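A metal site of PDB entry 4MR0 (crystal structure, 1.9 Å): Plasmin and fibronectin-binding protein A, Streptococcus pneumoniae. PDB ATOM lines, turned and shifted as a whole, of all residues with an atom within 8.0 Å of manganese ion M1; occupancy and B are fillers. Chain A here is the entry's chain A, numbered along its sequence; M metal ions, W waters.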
ATOM      1  N   ILE A 192      -0.193   3.038  12.233  1.00  0.00           N
ATOM      2  CA  ILE A 192      -0.970   3.662  11.166  1.00  0.00           C
ATOM      3  C   ILE A 192       0.038   4.470  10.355  1.00  0.00           C
ATOM      4  O   ILE A 192       0.759   5.295  10.912  1.00  0.00           O
ATOM      5  CB  ILE A 192      -2.050   4.584  11.772  1.00  0.00           C
ATOM      6  CG1 ILE A 192      -2.978   3.742  12.658  1.00  0.00           C
ATOM      7  CG2 ILE A 192      -2.824   5.300  10.656  1.00  0.00           C
ATOM      8  CD1 ILE A 192      -4.011   4.551  13.450  1.00  0.00           C
ATOM      9  N   HIS A 268      -8.498  -0.273  11.648  1.00  0.00           N
ATOM     10  CA  HIS A 268      -9.197   0.613  10.723  1.00  0.00           C
ATOM     11  C   HIS A 268      -8.237   1.031   9.628  1.00  0.00           C
ATOM     12  O   HIS A 268      -7.184   1.600   9.916  1.00  0.00           O
ATOM     13  CB  HIS A 268      -9.654   1.891  11.449  1.00  0.00           C
ATOM     14  CG  HIS A 268     -10.427   1.636  12.698  1.00  0.00           C
ATOM     15  ND1 HIS A 268     -11.680   1.063  12.691  1.00  0.00           N
ATOM     16  CD2 HIS A 268     -10.153   1.921  13.988  1.00  0.00           C
ATOM     17  CE1 HIS A 268     -12.147   1.007  13.930  1.00  0.00           C
ATOM     18  NE2 HIS A 268     -11.231   1.527  14.737  1.00  0.00           N
ATOM     19  N   ILE A 270      -8.887   3.265   7.556  1.00  0.00           N
ATOM     20  CA  ILE A 270      -9.041   4.706   7.575  1.00  0.00           C
ATOM     21  C   ILE A 270      -9.943   5.165   8.703  1.00  0.00           C
ATOM     22  O   ILE A 270     -10.989   4.581   8.942  1.00  0.00           O
ATOM     23  CB  ILE A 270      -9.663   5.212   6.245  1.00  0.00           C
ATOM     24  CG1 ILE A 270      -8.762   4.869   5.064  1.00  0.00           C
ATOM     25  CG2 ILE A 270      -9.905   6.725   6.321  1.00  0.00           C
ATOM     26  CD1 ILE A 270      -9.400   5.158   3.698  1.00  0.00           C
ATOM     27  N   GLN A 271      -9.529   6.228   9.399  1.00  0.00           N
ATOM     28  CA  GLN A 271     -10.349   6.820  10.454  1.00  0.00           C
ATOM     29  C   GLN A 271     -10.501   8.289  10.070  1.00  0.00           C
ATOM     30  O   GLN A 271      -9.515   8.985   9.850  1.00  0.00           O
ATOM     31  CB  GLN A 271      -9.674   6.723  11.827  1.00  0.00           C
ATOM     32  CG  GLN A 271      -9.622   5.312  12.396  1.00  0.00           C
ATOM     33  CD  GLN A 271      -8.882   5.258  13.720  1.00  0.00           C
ATOM     34  OE1 GLN A 271      -9.403   5.651  14.766  1.00  0.00           O
ATOM     35  NE2 GLN A 271      -7.649   4.770  13.686  1.00  0.00           N
ATOM     36  N   ILE A 272     -11.743   8.731   9.990  1.00  0.00           N
ATOM     37  CA  ILE A 272     -12.065  10.101   9.639  1.00  0.00           C
ATOM     38  C   ILE A 272     -12.794  10.646  10.851  1.00  0.00           C
ATOM     39  O   ILE A 272     -13.931  10.267  11.118  1.00  0.00           O
ATOM     40  CB  ILE A 272     -13.006  10.140   8.400  1.00  0.00           C
ATOM     41  CG1 ILE A 272     -12.306   9.462   7.216  1.00  0.00           C
ATOM     42  CG2 ILE A 272     -13.386  11.573   8.052  1.00  0.00           C
ATOM     43  CD1 ILE A 272     -13.239   9.173   6.038  1.00  0.00           C
ATOM     44  N   ALA A 273     -12.118  11.528  11.584  1.00  0.00           N
ATOM     45  CA  ALA A 273     -12.659  12.089  12.819  1.00  0.00           C
ATOM     46  C   ALA A 273     -12.642  13.603  12.823  1.00  0.00           C
ATOM     47  O   ALA A 273     -11.601  14.221  12.596  1.00  0.00           O
ATOM     48  CB  ALA A 273     -11.842  11.567  14.013  1.00  0.00           C
ATOM     49  N   SER A 301     -15.947  -3.989  16.426  1.00  0.00           N
ATOM     50  CA  SER A 301     -15.678  -2.570  16.613  1.00  0.00           C
ATOM     51  C   SER A 301     -14.556  -2.132  15.669  1.00  0.00           C
ATOM     52  O   SER A 301     -14.025  -1.024  15.788  1.00  0.00           O
ATOM     53  CB  SER A 301     -15.251  -2.300  18.054  1.00  0.00           C
ATOM     54  OG  SER A 301     -13.982  -2.849  18.315  1.00  0.00           O
ATOM     55  N   GLU A 303     -14.125  -1.271  12.077  1.00  0.00           N
ATOM     56  CA  GLU A 303     -14.582  -0.914  10.734  1.00  0.00           C
ATOM     57  C   GLU A 303     -13.373  -0.553   9.882  1.00  0.00           C
ATOM     58  O   GLU A 303     -12.455   0.104  10.357  1.00  0.00           O
ATOM     59  CB  GLU A 303     -15.535   0.286  10.801  1.00  0.00           C
ATOM     60  CG  GLU A 303     -16.742   0.116  11.719  1.00  0.00           C
ATOM     61  CD  GLU A 303     -16.480   0.593  13.146  1.00  0.00           C
ATOM     62  OE1 GLU A 303     -15.325   0.933  13.471  1.00  0.00           O
ATOM     63  OE2 GLU A 303     -17.443   0.610  13.939  1.00  0.00           O
ATOM     64  N   GLN A 306     -13.803   4.028   9.385  1.00  0.00           N
ATOM     65  CA  GLN A 306     -14.594   4.529  10.490  1.00  0.00           C
ATOM     66  C   GLN A 306     -14.770   6.037  10.307  1.00  0.00           C
ATOM     67  O   GLN A 306     -13.831   6.750   9.988  1.00  0.00           O
ATOM     68  CB  GLN A 306     -13.885   4.241  11.823  1.00  0.00           C
ATOM     69  CG  GLN A 306     -14.602   4.771  13.057  1.00  0.00           C
ATOM     70  CD  GLN A 306     -13.849   4.443  14.336  1.00  0.00           C
ATOM     71  OE1 GLN A 306     -12.627   4.516  14.385  1.00  0.00           O
ATOM     72  NE2 GLN A 306     -14.591   4.096  15.383  1.00  0.00           N
ATOM     73  N   ILE A 307     -16.002   6.496  10.493  1.00  0.00           N
ATOM     74  CA  ILE A 307     -16.352   7.908  10.365  1.00  0.00           C
ATOM     75  C   ILE A 307     -16.893   8.226  11.749  1.00  0.00           C
ATOM     76  O   ILE A 307     -17.934   7.721  12.153  1.00  0.00           O
ATOM     77  CB  ILE A 307     -17.439   8.100   9.293  1.00  0.00           C
ATOM     78  CG1 ILE A 307     -16.923   7.561   7.958  1.00  0.00           C
ATOM     79  CG2 ILE A 307     -17.794   9.590   9.185  1.00  0.00           C
ATOM     80  CD1 ILE A 307     -18.016   7.443   6.888  1.00  0.00           C
ATOM     81  N   GLU A 308     -16.188   9.090  12.472  1.00  0.00           N
ATOM     82  CA  GLU A 308     -16.578   9.365  13.844  1.00  0.00           C
ATOM     83  C   GLU A 308     -16.334  10.808  14.267  1.00  0.00           C
ATOM     84  O   GLU A 308     -15.697  11.578  13.559  1.00  0.00           O
ATOM     85  CB  GLU A 308     -15.751   8.460  14.741  1.00  0.00           C
ATOM     86  CG  GLU A 308     -14.258   8.849  14.689  1.00  0.00           C
ATOM     87  CD  GLU A 308     -13.315   7.775  15.200  1.00  0.00           C
ATOM     88  OE1 GLU A 308     -13.631   7.126  16.216  1.00  0.00           O
ATOM     89  OE2 GLU A 308     -12.241   7.599  14.577  1.00  0.00           O
ATOM     90  N   PRO A 309     -16.884  11.187  15.430  1.00  0.00           N
ATOM     91  CA  PRO A 309     -16.676  12.554  15.925  1.00  0.00           C
ATOM     92  C   PRO A 309     -15.276  12.520  16.523  1.00  0.00           C
ATOM     93  O   PRO A 309     -14.712  11.444  16.739  1.00  0.00           O
ATOM     94  CB  PRO A 309     -17.784  12.718  16.975  1.00  0.00           C
ATOM     95  CG  PRO A 309     -18.032  11.325  17.444  1.00  0.00           C
ATOM     96  CD  PRO A 309     -17.978  10.512  16.160  1.00  0.00           C
ATOM     97  N   THR A 311     -12.937  12.601  19.413  1.00  0.00           N
ATOM     98  CA  THR A 311     -12.776  12.451  20.855  1.00  0.00           C
ATOM     99  C   THR A 311     -11.522  11.621  21.098  1.00  0.00           C
ATOM    100  O   THR A 311     -11.063  10.914  20.209  1.00  0.00           O
ATOM    101  CB  THR A 311     -13.976  11.711  21.515  1.00  0.00           C
ATOM    102  OG1 THR A 311     -13.981  10.337  21.095  1.00  0.00           O
ATOM    103  CG2 THR A 311     -15.293  12.369  21.119  1.00  0.00           C
ATOM    104  N   ARG A 312     -10.962  11.706  22.296  1.00  0.00           N
ATOM    105  CA  ARG A 312      -9.756  10.945  22.599  1.00  0.00           C
ATOM    106  C   ARG A 312     -10.063   9.445  22.632  1.00  0.00           C
ATOM    107  O   ARG A 312      -9.212   8.623  22.272  1.00  0.00           O
ATOM    108  CB  ARG A 312      -9.166  11.430  23.929  1.00  0.00           C
ATOM    109  CG  ARG A 312      -8.676  12.867  23.851  1.00  0.00           C
ATOM    110  CD  ARG A 312      -8.176  13.415  25.183  1.00  0.00           C
ATOM    111  NE  ARG A 312      -6.942  12.756  25.623  1.00  0.00           N
ATOM    112  CZ  ARG A 312      -6.286  13.096  26.729  1.00  0.00           C
ATOM    113  NH1 ARG A 312      -6.731  14.080  27.494  1.00  0.00           N
ATOM    114  NH2 ARG A 312      -5.176  12.449  27.071  1.00  0.00           N
ATOM    115  N   LYS A 313     -11.284   9.096  23.030  1.00  0.00           N
ATOM    116  CA  LYS A 313     -11.704   7.703  23.082  1.00  0.00           C
ATOM    117  C   LYS A 313     -11.669   7.059  21.697  1.00  0.00           C
ATOM    118  O   LYS A 313     -11.129   5.968  21.525  1.00  0.00           O
ATOM    119  CB  LYS A 313     -13.122   7.611  23.661  1.00  0.00           C
ATOM    120  CG  LYS A 313     -13.709   6.206  23.689  1.00  0.00           C
ATOM    121  CD  LYS A 313     -12.996   5.315  24.691  1.00  0.00           C
ATOM    122  CE  LYS A 313     -13.496   3.866  24.607  1.00  0.00           C
ATOM    123  NZ  LYS A 313     -14.981   3.774  24.774  1.00  0.00           N
ATOM    124  N   GLY A 314     -12.238   7.735  20.702  1.00  0.00           N
ATOM    125  CA  GLY A 314     -12.228   7.190  19.358  1.00  0.00           C
ATOM    126  C   GLY A 314     -11.043   7.623  18.505  1.00  0.00           C
ATOM    127  O   GLY A 314     -10.790   7.048  17.458  1.00  0.00           O
ATOM    128  N   PHE A 315     -10.303   8.634  18.952  1.00  0.00           N
ATOM    129  CA  PHE A 315      -9.153   9.122  18.180  1.00  0.00           C
ATOM    130  C   PHE A 315      -8.044   9.452  19.182  1.00  0.00           C
ATOM    131  O   PHE A 315      -7.737  10.620  19.431  1.00  0.00           O
ATOM    132  CB  PHE A 315      -9.577  10.366  17.379  1.00  0.00           C
ATOM    133  CG  PHE A 315      -8.748  10.618  16.159  1.00  0.00           C
ATOM    134  CD1 PHE A 315      -8.930   9.859  15.008  1.00  0.00           C
ATOM    135  CD2 PHE A 315      -7.766  11.610  16.162  1.00  0.00           C
ATOM    136  CE1 PHE A 315      -8.145  10.093  13.870  1.00  0.00           C
ATOM    137  CE2 PHE A 315      -6.982  11.854  15.041  1.00  0.00           C
ATOM    138  CZ  PHE A 315      -7.177  11.085  13.884  1.00  0.00           C
ATOM    139  N   PRO A 316      -7.425   8.418  19.769  1.00  0.00           N
ATOM    140  CA  PRO A 316      -6.346   8.542  20.763  1.00  0.00           C
ATOM    141  C   PRO A 316      -5.018   9.105  20.275  1.00  0.00           C
ATOM    142  O   PRO A 316      -4.053   9.171  21.050  1.00  0.00           O
ATOM    143  CB  PRO A 316      -6.225   7.119  21.295  1.00  0.00           C
ATOM    144  CG  PRO A 316      -6.502   6.301  20.071  1.00  0.00           C
ATOM    145  CD  PRO A 316      -7.695   7.006  19.457  1.00  0.00           C
ATOM    146  N   TYR A 317      -4.961   9.534  19.031  1.00  0.00           N
ATOM    147  CA  TYR A 317      -3.736  10.060  18.442  1.00  0.00           C
ATOM    148  C   TYR A 317      -3.508  11.537  18.733  1.00  0.00           C
ATOM    149  O   TYR A 317      -2.428  12.073  18.479  1.00  0.00           O
ATOM    150  CB  TYR A 317      -3.757   9.834  16.933  1.00  0.00           C
ATOM    151  CG  TYR A 317      -4.354   8.487  16.596  1.00  0.00           C
ATOM    152  CD1 TYR A 317      -3.702   7.318  16.975  1.00  0.00           C
ATOM    153  CD2 TYR A 317      -5.605   8.390  15.985  1.00  0.00           C
ATOM    154  CE1 TYR A 317      -4.293   6.065  16.769  1.00  0.00           C
ATOM    155  CE2 TYR A 317      -6.203   7.147  15.772  1.00  0.00           C
ATOM    156  CZ  TYR A 317      -5.540   6.000  16.172  1.00  0.00           C
ATOM    157  OH  TYR A 317      -6.123   4.766  16.001  1.00  0.00           O
ATOM    158  N   GLY A 350     -18.493   2.572   8.962  1.00  0.00           N
ATOM    159  CA  GLY A 350     -19.388   2.910  10.063  1.00  0.00           C
ATOM    160  C   GLY A 350     -18.684   3.399  11.312  1.00  0.00           C
ATOM    161  O   GLY A 350     -17.592   3.939  11.248  1.00  0.00           O
ATOM    162  N   THR A 351     -19.356   3.226  12.439  1.00  0.00           N
ATOM    163  CA  THR A 351     -18.796   3.595  13.725  1.00  0.00           C
ATOM    164  C   THR A 351     -19.639   2.914  14.796  1.00  0.00           C
ATOM    165  O   THR A 351     -20.739   2.424  14.525  1.00  0.00           O
ATOM    166  CB  THR A 351     -18.727   5.123  13.938  1.00  0.00           C
ATOM    167  OG1 THR A 351     -17.855   5.397  15.037  1.00  0.00           O
ATOM    168  CG2 THR A 351     -20.108   5.696  14.208  1.00  0.00           C
ATOM    169  N   HIS A 352     -19.125   2.890  16.028  1.00  0.00           N
ATOM    170  CA  HIS A 352     -19.816   2.192  17.107  1.00  0.00           C
ATOM    171  C   HIS A 352     -19.807   2.953  18.428  1.00  0.00           C
ATOM    172  O   HIS A 352     -19.904   2.332  19.486  1.00  0.00           O
ATOM    173  CB  HIS A 352     -19.095   0.873  17.335  1.00  0.00           C
ATOM    174  CG  HIS A 352     -17.620   1.060  17.562  1.00  0.00           C
ATOM    175  ND1 HIS A 352     -16.718   1.173  16.523  1.00  0.00           N
ATOM    176  CD2 HIS A 352     -16.904   1.241  18.692  1.00  0.00           C
ATOM    177  CE1 HIS A 352     -15.516   1.422  17.007  1.00  0.00           C
ATOM    178  NE2 HIS A 352     -15.605   1.464  18.321  1.00  0.00           N
ATOM    179  N   TYR A 353     -19.711   4.273  18.373  1.00  0.00           N
ATOM    180  CA  TYR A 353     -19.643   5.033  19.613  1.00  0.00           C
ATOM    181  C   TYR A 353     -20.212   6.433  19.507  1.00  0.00           C
ATOM    182  O   TYR A 353     -20.036   7.116  18.496  1.00  0.00           O
ATOM    183  CB  TYR A 353     -18.172   5.091  20.046  1.00  0.00           C
ATOM    184  CG  TYR A 353     -17.880   5.928  21.271  1.00  0.00           C
ATOM    185  CD1 TYR A 353     -18.219   5.491  22.542  1.00  0.00           C
ATOM    186  CD2 TYR A 353     -17.213   7.154  21.150  1.00  0.00           C
ATOM    187  CE1 TYR A 353     -17.900   6.239  23.684  1.00  0.00           C
ATOM    188  CE2 TYR A 353     -16.887   7.918  22.281  1.00  0.00           C
ATOM    189  CZ  TYR A 353     -17.232   7.448  23.538  1.00  0.00           C
ATOM    190  OH  TYR A 353     -16.908   8.192  24.658  1.00  0.00           O
HETATM  191 MN    MN M   1     -11.466   5.815  15.791  1.00  0.00          MN
HETATM  192 MN    MN M   2     -11.839   3.567  17.893  1.00  0.00          MN
HETATM  193  O   HOH W   1     -13.871   4.402  17.740  1.00  0.00           O
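N of Glu 308 is in hydrogen-bond range of O of Ile 272, 2.9 Å away.
NE2 of Gln 271 lies within hydrogen-bond range of OH of Tyr 317 (2.8 Å).
N of Gly 314 sits at hydrogen-bond distance from OG1 of Thr 311, at 3.2 Å.
The backbone carbonyl oxygen (O) of Ile 270 is in hydrogen-bond range of the backbone NH (N) of Gln 306.
The backbone carbonyl oxygen (O) of Gln 306 lies within hydrogen-bond range of the backbone NH (N) of Ile 272, 2.9 Å away.
OE1 of Gln 306 lies close to NE2 of His 268, at 3.3 Å.
Manganese ion M1 is bound by O of Gly 314, 2.2 Å away.
OE1 of Gln 306 binds manganese ion M1, 2.2 Å away.
OE2 of Glu 308 is bound to manganese ion M1, 2.3 Å away.
OE1 of Gln 271 binds manganese ion M1 (2.3 Å).
OE1 of Glu 308 is bound to manganese ion M1.
Water W1 lies within hydrogen-bond range of NE2 of Gln 306 (2.5 Å) and NE2 of His 352 (3.5 Å).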
